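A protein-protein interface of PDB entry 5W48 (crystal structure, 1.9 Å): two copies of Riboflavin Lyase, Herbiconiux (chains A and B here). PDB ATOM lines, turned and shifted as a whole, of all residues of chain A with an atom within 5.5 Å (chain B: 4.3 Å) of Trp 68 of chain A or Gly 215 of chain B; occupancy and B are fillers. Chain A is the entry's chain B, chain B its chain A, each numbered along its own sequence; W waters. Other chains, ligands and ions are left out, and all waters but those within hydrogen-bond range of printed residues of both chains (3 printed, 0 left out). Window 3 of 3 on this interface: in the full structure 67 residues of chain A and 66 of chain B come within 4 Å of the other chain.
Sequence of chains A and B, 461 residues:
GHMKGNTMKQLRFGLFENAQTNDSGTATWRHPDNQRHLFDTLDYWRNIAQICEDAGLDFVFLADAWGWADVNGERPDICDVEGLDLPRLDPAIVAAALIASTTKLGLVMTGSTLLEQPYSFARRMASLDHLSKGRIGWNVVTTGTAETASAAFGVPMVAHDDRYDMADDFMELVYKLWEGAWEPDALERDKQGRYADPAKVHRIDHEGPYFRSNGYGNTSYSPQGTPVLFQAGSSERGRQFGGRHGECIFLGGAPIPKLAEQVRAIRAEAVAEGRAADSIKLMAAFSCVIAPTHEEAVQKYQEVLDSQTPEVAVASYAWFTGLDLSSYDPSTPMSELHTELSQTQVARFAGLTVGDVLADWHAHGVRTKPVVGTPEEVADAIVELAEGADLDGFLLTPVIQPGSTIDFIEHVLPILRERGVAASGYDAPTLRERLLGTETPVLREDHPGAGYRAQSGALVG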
ATOM      1  N   TRP A  66       8.372   3.589  23.832  1.00  0.00           N
ATOM      2  CA  TRP A  66       9.075   4.611  23.077  1.00  0.00           C
ATOM      3  C   TRP A  66      10.481   4.196  22.682  1.00  0.00           C
ATOM      4  O   TRP A  66      11.039   4.778  21.749  1.00  0.00           O
ATOM      5  CB  TRP A  66       9.152   5.912  23.883  1.00  0.00           C
ATOM      6  CG  TRP A  66       7.840   6.630  23.989  1.00  0.00           C
ATOM      7  CD1 TRP A  66       6.947   6.578  25.031  1.00  0.00           C
ATOM      8  CD2 TRP A  66       7.264   7.497  23.012  1.00  0.00           C
ATOM      9  NE1 TRP A  66       5.861   7.369  24.757  1.00  0.00           N
ATOM     10  CE2 TRP A  66       6.033   7.951  23.529  1.00  0.00           C
ATOM     11  CE3 TRP A  66       7.673   7.941  21.752  1.00  0.00           C
ATOM     12  CZ2 TRP A  66       5.208   8.824  22.832  1.00  0.00           C
ATOM     13  CZ3 TRP A  66       6.851   8.807  21.059  1.00  0.00           C
ATOM     14  CH2 TRP A  66       5.628   9.234  21.598  1.00  0.00           C
ATOM     15  N   GLY A  67      11.055   3.209  23.358  1.00  0.00           N
ATOM     16  CA  GLY A  67      12.432   2.817  23.140  1.00  0.00           C
ATOM     17  C   GLY A  67      12.601   1.731  22.097  1.00  0.00           C
ATOM     18  O   GLY A  67      11.755   1.525  21.222  1.00  0.00           O
ATOM     19  N   TRP A  68      13.734   1.042  22.194  1.00  0.00           N
ATOM     20  CA  TRP A  68      14.119  -0.027  21.279  1.00  0.00           C
ATOM     21  C   TRP A  68      15.094  -0.936  22.013  1.00  0.00           C
ATOM     22  O   TRP A  68      15.532  -0.640  23.127  1.00  0.00           O
ATOM     23  CB  TRP A  68      14.755   0.529  19.995  1.00  0.00           C
ATOM     24  CG  TRP A  68      15.892   1.491  20.279  1.00  0.00           C
ATOM     25  CD1 TRP A  68      17.207   1.180  20.480  1.00  0.00           C
ATOM     26  CD2 TRP A  68      15.789   2.919  20.408  1.00  0.00           C
ATOM     27  NE1 TRP A  68      17.925   2.321  20.727  1.00  0.00           N
ATOM     28  CE2 TRP A  68      17.078   3.403  20.683  1.00  0.00           C
ATOM     29  CE3 TRP A  68      14.722   3.830  20.320  1.00  0.00           C
ATOM     30  CZ2 TRP A  68      17.343   4.761  20.872  1.00  0.00           C
ATOM     31  CZ3 TRP A  68      14.985   5.177  20.498  1.00  0.00           C
ATOM     32  CH2 TRP A  68      16.287   5.630  20.775  1.00  0.00           C
ATOM     33  N   ALA A  69      15.457  -2.035  21.360  1.00  0.00           N
ATOM     34  CA  ALA A  69      16.295  -3.041  21.997  1.00  0.00           C
ATOM     35  C   ALA A  69      17.744  -2.587  22.137  1.00  0.00           C
ATOM     36  O   ALA A  69      18.329  -1.987  21.228  1.00  0.00           O
ATOM     37  CB  ALA A  69      16.244  -4.353  21.217  1.00  0.00           C
ATOM     38  N   ASP A  70      18.318  -2.895  23.292  1.00  0.00           N
ATOM     39  CA  ASP A  70      19.713  -2.628  23.617  1.00  0.00           C
ATOM     40  C   ASP A  70      20.311  -3.937  24.109  1.00  0.00           C
ATOM     41  O   ASP A  70      19.859  -4.478  25.121  1.00  0.00           O
ATOM     42  CB  ASP A  70      19.818  -1.537  24.693  1.00  0.00           C
ATOM     43  CG  ASP A  70      21.259  -1.209  25.090  1.00  0.00           C
ATOM     44  OD1 ASP A  70      22.126  -2.108  25.106  1.00  0.00           O
ATOM     45  OD2 ASP A  70      21.523  -0.029  25.409  1.00  0.00           O
ATOM     46  N   ARG A  75      21.956  -2.088  19.027  1.00  0.00           N
ATOM     47  CA  ARG A  75      20.736  -2.712  18.536  1.00  0.00           C
ATOM     48  C   ARG A  75      21.145  -3.727  17.474  1.00  0.00           C
ATOM     49  O   ARG A  75      21.476  -3.334  16.344  1.00  0.00           O
ATOM     50  CB  ARG A  75      19.767  -1.673  17.958  1.00  0.00           C
ATOM     51  CG  ARG A  75      18.419  -2.262  17.564  1.00  0.00           C
ATOM     52  CD  ARG A  75      17.410  -1.205  17.133  1.00  0.00           C
ATOM     53  NE  ARG A  75      16.174  -1.835  16.678  1.00  0.00           N
ATOM     54  CZ  ARG A  75      15.925  -2.171  15.415  1.00  0.00           C
ATOM     55  NH1 ARG A  75      16.821  -1.916  14.473  1.00  0.00           N
ATOM     56  NH2 ARG A  75      14.778  -2.758  15.094  1.00  0.00           N
ATOM     57  N   ASP A  85      11.426  -5.270  18.179  1.00  0.00           N
ATOM     58  CA  ASP A  85      11.141  -4.050  18.933  1.00  0.00           C
ATOM     59  C   ASP A  85      10.405  -2.997  18.108  1.00  0.00           C
ATOM     60  O   ASP A  85       9.590  -2.240  18.648  1.00  0.00           O
ATOM     61  CB  ASP A  85      12.445  -3.454  19.501  1.00  0.00           C
ATOM     62  CG  ASP A  85      13.537  -3.218  18.433  1.00  0.00           C
ATOM     63  OD1 ASP A  85      13.459  -3.760  17.305  1.00  0.00           O
ATOM     64  OD2 ASP A  85      14.512  -2.490  18.748  1.00  0.00           O
ATOM     65  N   LEU A  86      10.669  -2.960  16.807  1.00  0.00           N
ATOM     66  CA  LEU A  86      10.237  -1.854  15.945  1.00  0.00           C
ATOM     67  C   LEU A  86       9.868  -2.410  14.577  1.00  0.00           C
ATOM     68  O   LEU A  86      10.350  -3.468  14.196  1.00  0.00           O
ATOM     69  CB  LEU A  86      11.356  -0.813  15.806  1.00  0.00           C
ATOM     70  CG  LEU A  86      11.856  -0.016  17.009  1.00  0.00           C
ATOM     71  CD1 LEU A  86      13.091   0.768  16.577  1.00  0.00           C
ATOM     72  CD2 LEU A  86      10.803   0.908  17.512  1.00  0.00           C
ATOM     73  N   ARG A  88       6.518   0.659  15.184  1.00  0.00           N
ATOM     74  CA  ARG A  88       5.247   0.663  15.899  1.00  0.00           C
ATOM     75  C   ARG A  88       4.443   1.885  15.475  1.00  0.00           C
ATOM     76  O   ARG A  88       4.939   2.759  14.761  1.00  0.00           O
ATOM     77  CB  ARG A  88       5.452   0.622  17.424  1.00  0.00           C
ATOM     78  CG  ARG A  88       6.242   1.772  18.032  1.00  0.00           C
ATOM     79  CD  ARG A  88       6.427   1.557  19.552  1.00  0.00           C
ATOM     80  NE  ARG A  88       7.421   0.527  19.896  1.00  0.00           N
ATOM     81  CZ  ARG A  88       8.636   0.791  20.381  1.00  0.00           C
ATOM     82  NH1 ARG A  88       9.018   2.041  20.580  1.00  0.00           N
ATOM     83  NH2 ARG A  88       9.477  -0.187  20.669  1.00  0.00           N
ATOM     84  N   THR A 148      17.156   4.928  26.374  1.00  0.00           N
ATOM     85  CA  THR A 148      16.790   5.068  24.965  1.00  0.00           C
ATOM     86  C   THR A 148      15.675   6.086  24.783  1.00  0.00           C
ATOM     87  O   THR A 148      15.825   7.062  24.040  1.00  0.00           O
ATOM     88  CB  THR A 148      16.382   3.720  24.362  1.00  0.00           C
ATOM     89  OG1 THR A 148      15.230   3.206  25.038  1.00  0.00           O
ATOM     90  CG2 THR A 148      17.530   2.719  24.442  1.00  0.00           C
ATOM     91  N   ALA A 149      14.541   5.871  25.448  1.00  0.00           N
ATOM     92  CA  ALA A 149      13.418   6.783  25.288  1.00  0.00           C
ATOM     93  C   ALA A 149      13.821   8.230  25.580  1.00  0.00           C
ATOM     94  O   ALA A 149      13.325   9.153  24.929  1.00  0.00           O
ATOM     95  CB  ALA A 149      12.259   6.332  26.183  1.00  0.00           C
ATOM     96  N   ALA A 151      17.041   9.544  25.256  1.00  0.00           N
ATOM     97  CA  ALA A 151      17.899  10.027  24.173  1.00  0.00           C
ATOM     98  C   ALA A 151      17.089  10.413  22.936  1.00  0.00           C
ATOM     99  O   ALA A 151      17.496  11.298  22.174  1.00  0.00           O
ATOM    100  CB  ALA A 151      18.928   8.964  23.804  1.00  0.00           C
ATOM    101  N   ALA A 152      15.953   9.753  22.716  1.00  0.00           N
ATOM    102  CA  ALA A 152      15.108  10.088  21.577  1.00  0.00           C
ATOM    103  C   ALA A 152      14.501  11.479  21.724  1.00  0.00           C
ATOM    104  O   ALA A 152      14.382  12.218  20.739  1.00  0.00           O
ATOM    105  CB  ALA A 152      14.012   9.035  21.424  1.00  0.00           C
ATOM    106  N   TRP A 319      18.220  -8.031  26.275  1.00  0.00           N
ATOM    107  CA  TRP A 319      17.573  -6.729  26.181  1.00  0.00           C
ATOM    108  C   TRP A 319      16.708  -6.453  27.410  1.00  0.00           C
ATOM    109  O   TRP A 319      16.790  -5.377  28.011  1.00  0.00           O
ATOM    110  CB  TRP A 319      16.758  -6.667  24.883  1.00  0.00           C
ATOM    111  CG  TRP A 319      15.723  -5.600  24.789  1.00  0.00           C
ATOM    112  CD1 TRP A 319      15.722  -4.376  25.402  1.00  0.00           C
ATOM    113  CD2 TRP A 319      14.520  -5.656  24.013  1.00  0.00           C
ATOM    114  NE1 TRP A 319      14.590  -3.678  25.065  1.00  0.00           N
ATOM    115  CE2 TRP A 319      13.835  -4.438  24.212  1.00  0.00           C
ATOM    116  CE3 TRP A 319      13.957  -6.618  23.169  1.00  0.00           C
ATOM    117  CZ2 TRP A 319      12.618  -4.155  23.597  1.00  0.00           C
ATOM    118  CZ3 TRP A 319      12.746  -6.338  22.559  1.00  0.00           C
ATOM    119  CH2 TRP A 319      12.088  -5.115  22.778  1.00  0.00           C
ATOM    120  N   TYR B 119       9.812  14.423  18.394  1.00  0.00           N
ATOM    121  CA  TYR B 119       9.894  12.969  18.296  1.00  0.00           C
ATOM    122  C   TYR B 119       8.517  12.325  18.393  1.00  0.00           C
ATOM    123  O   TYR B 119       8.194  11.416  17.622  1.00  0.00           O
ATOM    124  CB  TYR B 119      10.816  12.409  19.378  1.00  0.00           C
ATOM    125  CG  TYR B 119      11.179  10.956  19.156  1.00  0.00           C
ATOM    126  CD1 TYR B 119      12.267  10.599  18.344  1.00  0.00           C
ATOM    127  CD2 TYR B 119      10.433   9.936  19.747  1.00  0.00           C
ATOM    128  CE1 TYR B 119      12.612   9.262  18.148  1.00  0.00           C
ATOM    129  CE2 TYR B 119      10.779   8.589  19.557  1.00  0.00           C
ATOM    130  CZ  TYR B 119      11.853   8.264  18.746  1.00  0.00           C
ATOM    131  OH  TYR B 119      12.175   6.933  18.555  1.00  0.00           O
ATOM    132  N   ARG B 203      19.988   4.571  12.746  1.00  0.00           N
ATOM    133  CA  ARG B 203      19.956   5.498  13.863  1.00  0.00           C
ATOM    134  C   ARG B 203      20.033   6.924  13.318  1.00  0.00           C
ATOM    135  O   ARG B 203      20.688   7.172  12.314  1.00  0.00           O
ATOM    136  CB  ARG B 203      21.130   5.179  14.800  1.00  0.00           C
ATOM    137  CG  ARG B 203      21.394   6.170  15.910  1.00  0.00           C
ATOM    138  CD  ARG B 203      22.623   5.767  16.721  1.00  0.00           C
ATOM    139  NE  ARG B 203      22.374   4.560  17.497  1.00  0.00           N
ATOM    140  CZ  ARG B 203      21.911   4.563  18.743  1.00  0.00           C
ATOM    141  NH1 ARG B 203      21.700   3.421  19.378  1.00  0.00           N
ATOM    142  NH2 ARG B 203      21.663   5.710  19.355  1.00  0.00           N
ATOM    143  N   ILE B 204      19.329   7.864  13.935  1.00  0.00           N
ATOM    144  CA  ILE B 204      19.506   9.259  13.556  1.00  0.00           C
ATOM    145  C   ILE B 204      20.307   9.972  14.639  1.00  0.00           C
ATOM    146  O   ILE B 204      20.448   9.504  15.777  1.00  0.00           O
ATOM    147  CB  ILE B 204      18.183  10.010  13.285  1.00  0.00           C
ATOM    148  CG1 ILE B 204      17.393  10.172  14.579  1.00  0.00           C
ATOM    149  CG2 ILE B 204      17.392   9.295  12.212  1.00  0.00           C
ATOM    150  CD1 ILE B 204      16.576  11.468  14.629  1.00  0.00           C
ATOM    151  N   ASN B 214      18.834  11.328  19.450  1.00  0.00           N
ATOM    152  CA  ASN B 214      19.816  10.314  19.094  1.00  0.00           C
ATOM    153  C   ASN B 214      19.136   8.966  19.218  1.00  0.00           C
ATOM    154  O   ASN B 214      18.597   8.647  20.283  1.00  0.00           O
ATOM    155  CB  ASN B 214      21.048  10.362  20.008  1.00  0.00           C
ATOM    156  CG  ASN B 214      21.787  11.668  19.915  1.00  0.00           C
ATOM    157  OD1 ASN B 214      22.760  11.782  19.174  1.00  0.00           O
ATOM    158  ND2 ASN B 214      21.331  12.671  20.664  1.00  0.00           N
ATOM    159  N   GLY B 215      19.163   8.183  18.148  1.00  0.00           N
ATOM    160  CA  GLY B 215      18.635   6.841  18.220  1.00  0.00           C
ATOM    161  C   GLY B 215      17.704   6.555  17.072  1.00  0.00           C
ATOM    162  O   GLY B 215      17.730   7.229  16.035  1.00  0.00           O
ATOM    163  N   TYR B 216      16.858   5.556  17.265  1.00  0.00           N
ATOM    164  CA  TYR B 216      16.027   5.067  16.179  1.00  0.00           C
ATOM    165  C   TYR B 216      14.685   5.781  16.163  1.00  0.00           C
ATOM    166  O   TYR B 216      14.267   6.373  17.158  1.00  0.00           O
ATOM    167  CB  TYR B 216      15.847   3.555  16.305  1.00  0.00           C
ATOM    168  CG  TYR B 216      17.158   2.837  16.067  1.00  0.00           C
ATOM    169  CD1 TYR B 216      18.097   2.719  17.081  1.00  0.00           C
ATOM    170  CD2 TYR B 216      17.476   2.341  14.814  1.00  0.00           C
ATOM    171  CE1 TYR B 216      19.306   2.089  16.866  1.00  0.00           C
ATOM    172  CE2 TYR B 216      18.692   1.716  14.589  1.00  0.00           C
ATOM    173  CZ  TYR B 216      19.597   1.590  15.624  1.00  0.00           C
ATOM    174  OH  TYR B 216      20.816   0.966  15.416  1.00  0.00           O
ATOM    175  N   GLY B 217      14.029   5.746  15.001  1.00  0.00           N
ATOM    176  CA  GLY B 217      12.673   6.263  14.870  1.00  0.00           C
ATOM    177  C   GLY B 217      11.647   5.163  15.117  1.00  0.00           C
ATOM    178  O   GLY B 217      11.858   4.012  14.756  1.00  0.00           O
HETATM  179  O   HOH W   1      20.711   2.698  22.179  1.00  0.00           O
HETATM  180  O   HOH W   2      19.611  12.772  22.801  1.00  0.00           O
HETATM  181  O   HOH W   3      20.123  -1.570  14.485  1.00  0.00           O
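Among the printed residues, pairs that only touch across the chains: Ala 152 of chain A with Tyr 119 of chain B (3.5 Å), Trp 68 of chain A with Tyr 216 of chain B (3.6 Å), Trp 68 of chain A with Gly 215 of chain B (3.6 Å), Ala 152 of chain A with Asn 214 of chain B (3.8 Å), Arg 75 of chain A with Tyr 216 of chain B (3.8 Å), Trp 68 of chain A with Asn 214 of chain B (3.8 Å), Trp 68 of chain A with Tyr 119 of chain B (3.8 Å), Trp 66 of chain A with Tyr 119 of chain B (3.9 Å), Leu 86 of chain A with Gly 217 of chain B (3.9 Å) and Leu 86 of chain A with Tyr 216 of chain B (3.9 Å).
N of Asn 214 of chain B lies within hydrogen-bond range of O of Ala 151 of chain A, at 3.0 Å.
Of the 14 printed residues of chain A, 6 touch a printed residue of chain B. Printed residues of chain A that touch a printed residue of chain B: Trp 66, Trp 68, Arg 75, Leu 86, Ala 151 and Ala 152. Hydrophobic or aromatic side chains of chain A that line the printed part of chain B: Trp 66, Trp 68, Leu 86, Ala 151 and Ala 152. Along chain A the printed residues that touch a printed residue of chain B span positions 66 to 152. Of the 7 printed residues of chain B, 5 touch a printed residue of chain A. Along chain B the printed residues that touch a printed residue of chain A span positions 119 to 217. Among the printed residues, 11 pairs touch across the chains.
NE of Arg 75 of chain A is in salt-bridge range of OD2 of Asp 85 of chain A (2.7 Å). The side-chain hydroxyl of Tyr 119 of chain B sits at hydrogen-bond distance from the backbone carbonyl oxygen of Tyr 216 of chain B (2.6 Å). The backbone NH (N) of Ile 204 of chain B is in hydrogen-bond range of the backbone carbonyl oxygen (O) of Gly 215 of chain B, 2.7 Å away.
Water W2 bridges O of Ala 151 of chain A (2.7 Å) and ND2 of Asn 214 of chain B (2.7 Å). Water W3 bridges OH of Tyr 216 of chain B and O of Arg 75 of chain A. Water W1 lies within hydrogen-bond range of NH1 of Arg 203 of chain B (3.1 Å) and NE1 of Trp 68 of chain A (3.2 Å).
No position is printed for both chains. Of the 11 pairs that touch across the chains among the printed residues, none has its exchanged pair printed and touching as well.
Trp 68 of chain A touches four residues of chain B. Gly 215 of chain B touches just one residue of chain A: Trp 68 (3.6 Å). Of the printed residues of chain A, Tyr 216 of chain B touches Trp 68, Arg 75 and Leu 86. Printed residues of chain B within 4 Å of Ala 152 of chain A: Tyr 119 (3.5 Å) and Asn 214 (3.8 Å). Of the printed residues of chain A, Asn 214 of chain B touches Trp 68, Ala 151 and Ala 152. Of the printed residues of chain A, Gly 217 of chain B touches Leu 86 (3.9 Å). Printed residues of chain B within 4 Å of Ala 151 of chain A: Asn 214 (3.0 Å). The nearest residue of chain A that does not touch Gly 215 of chain B is Ala 151 of chain A (5.4 Å).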
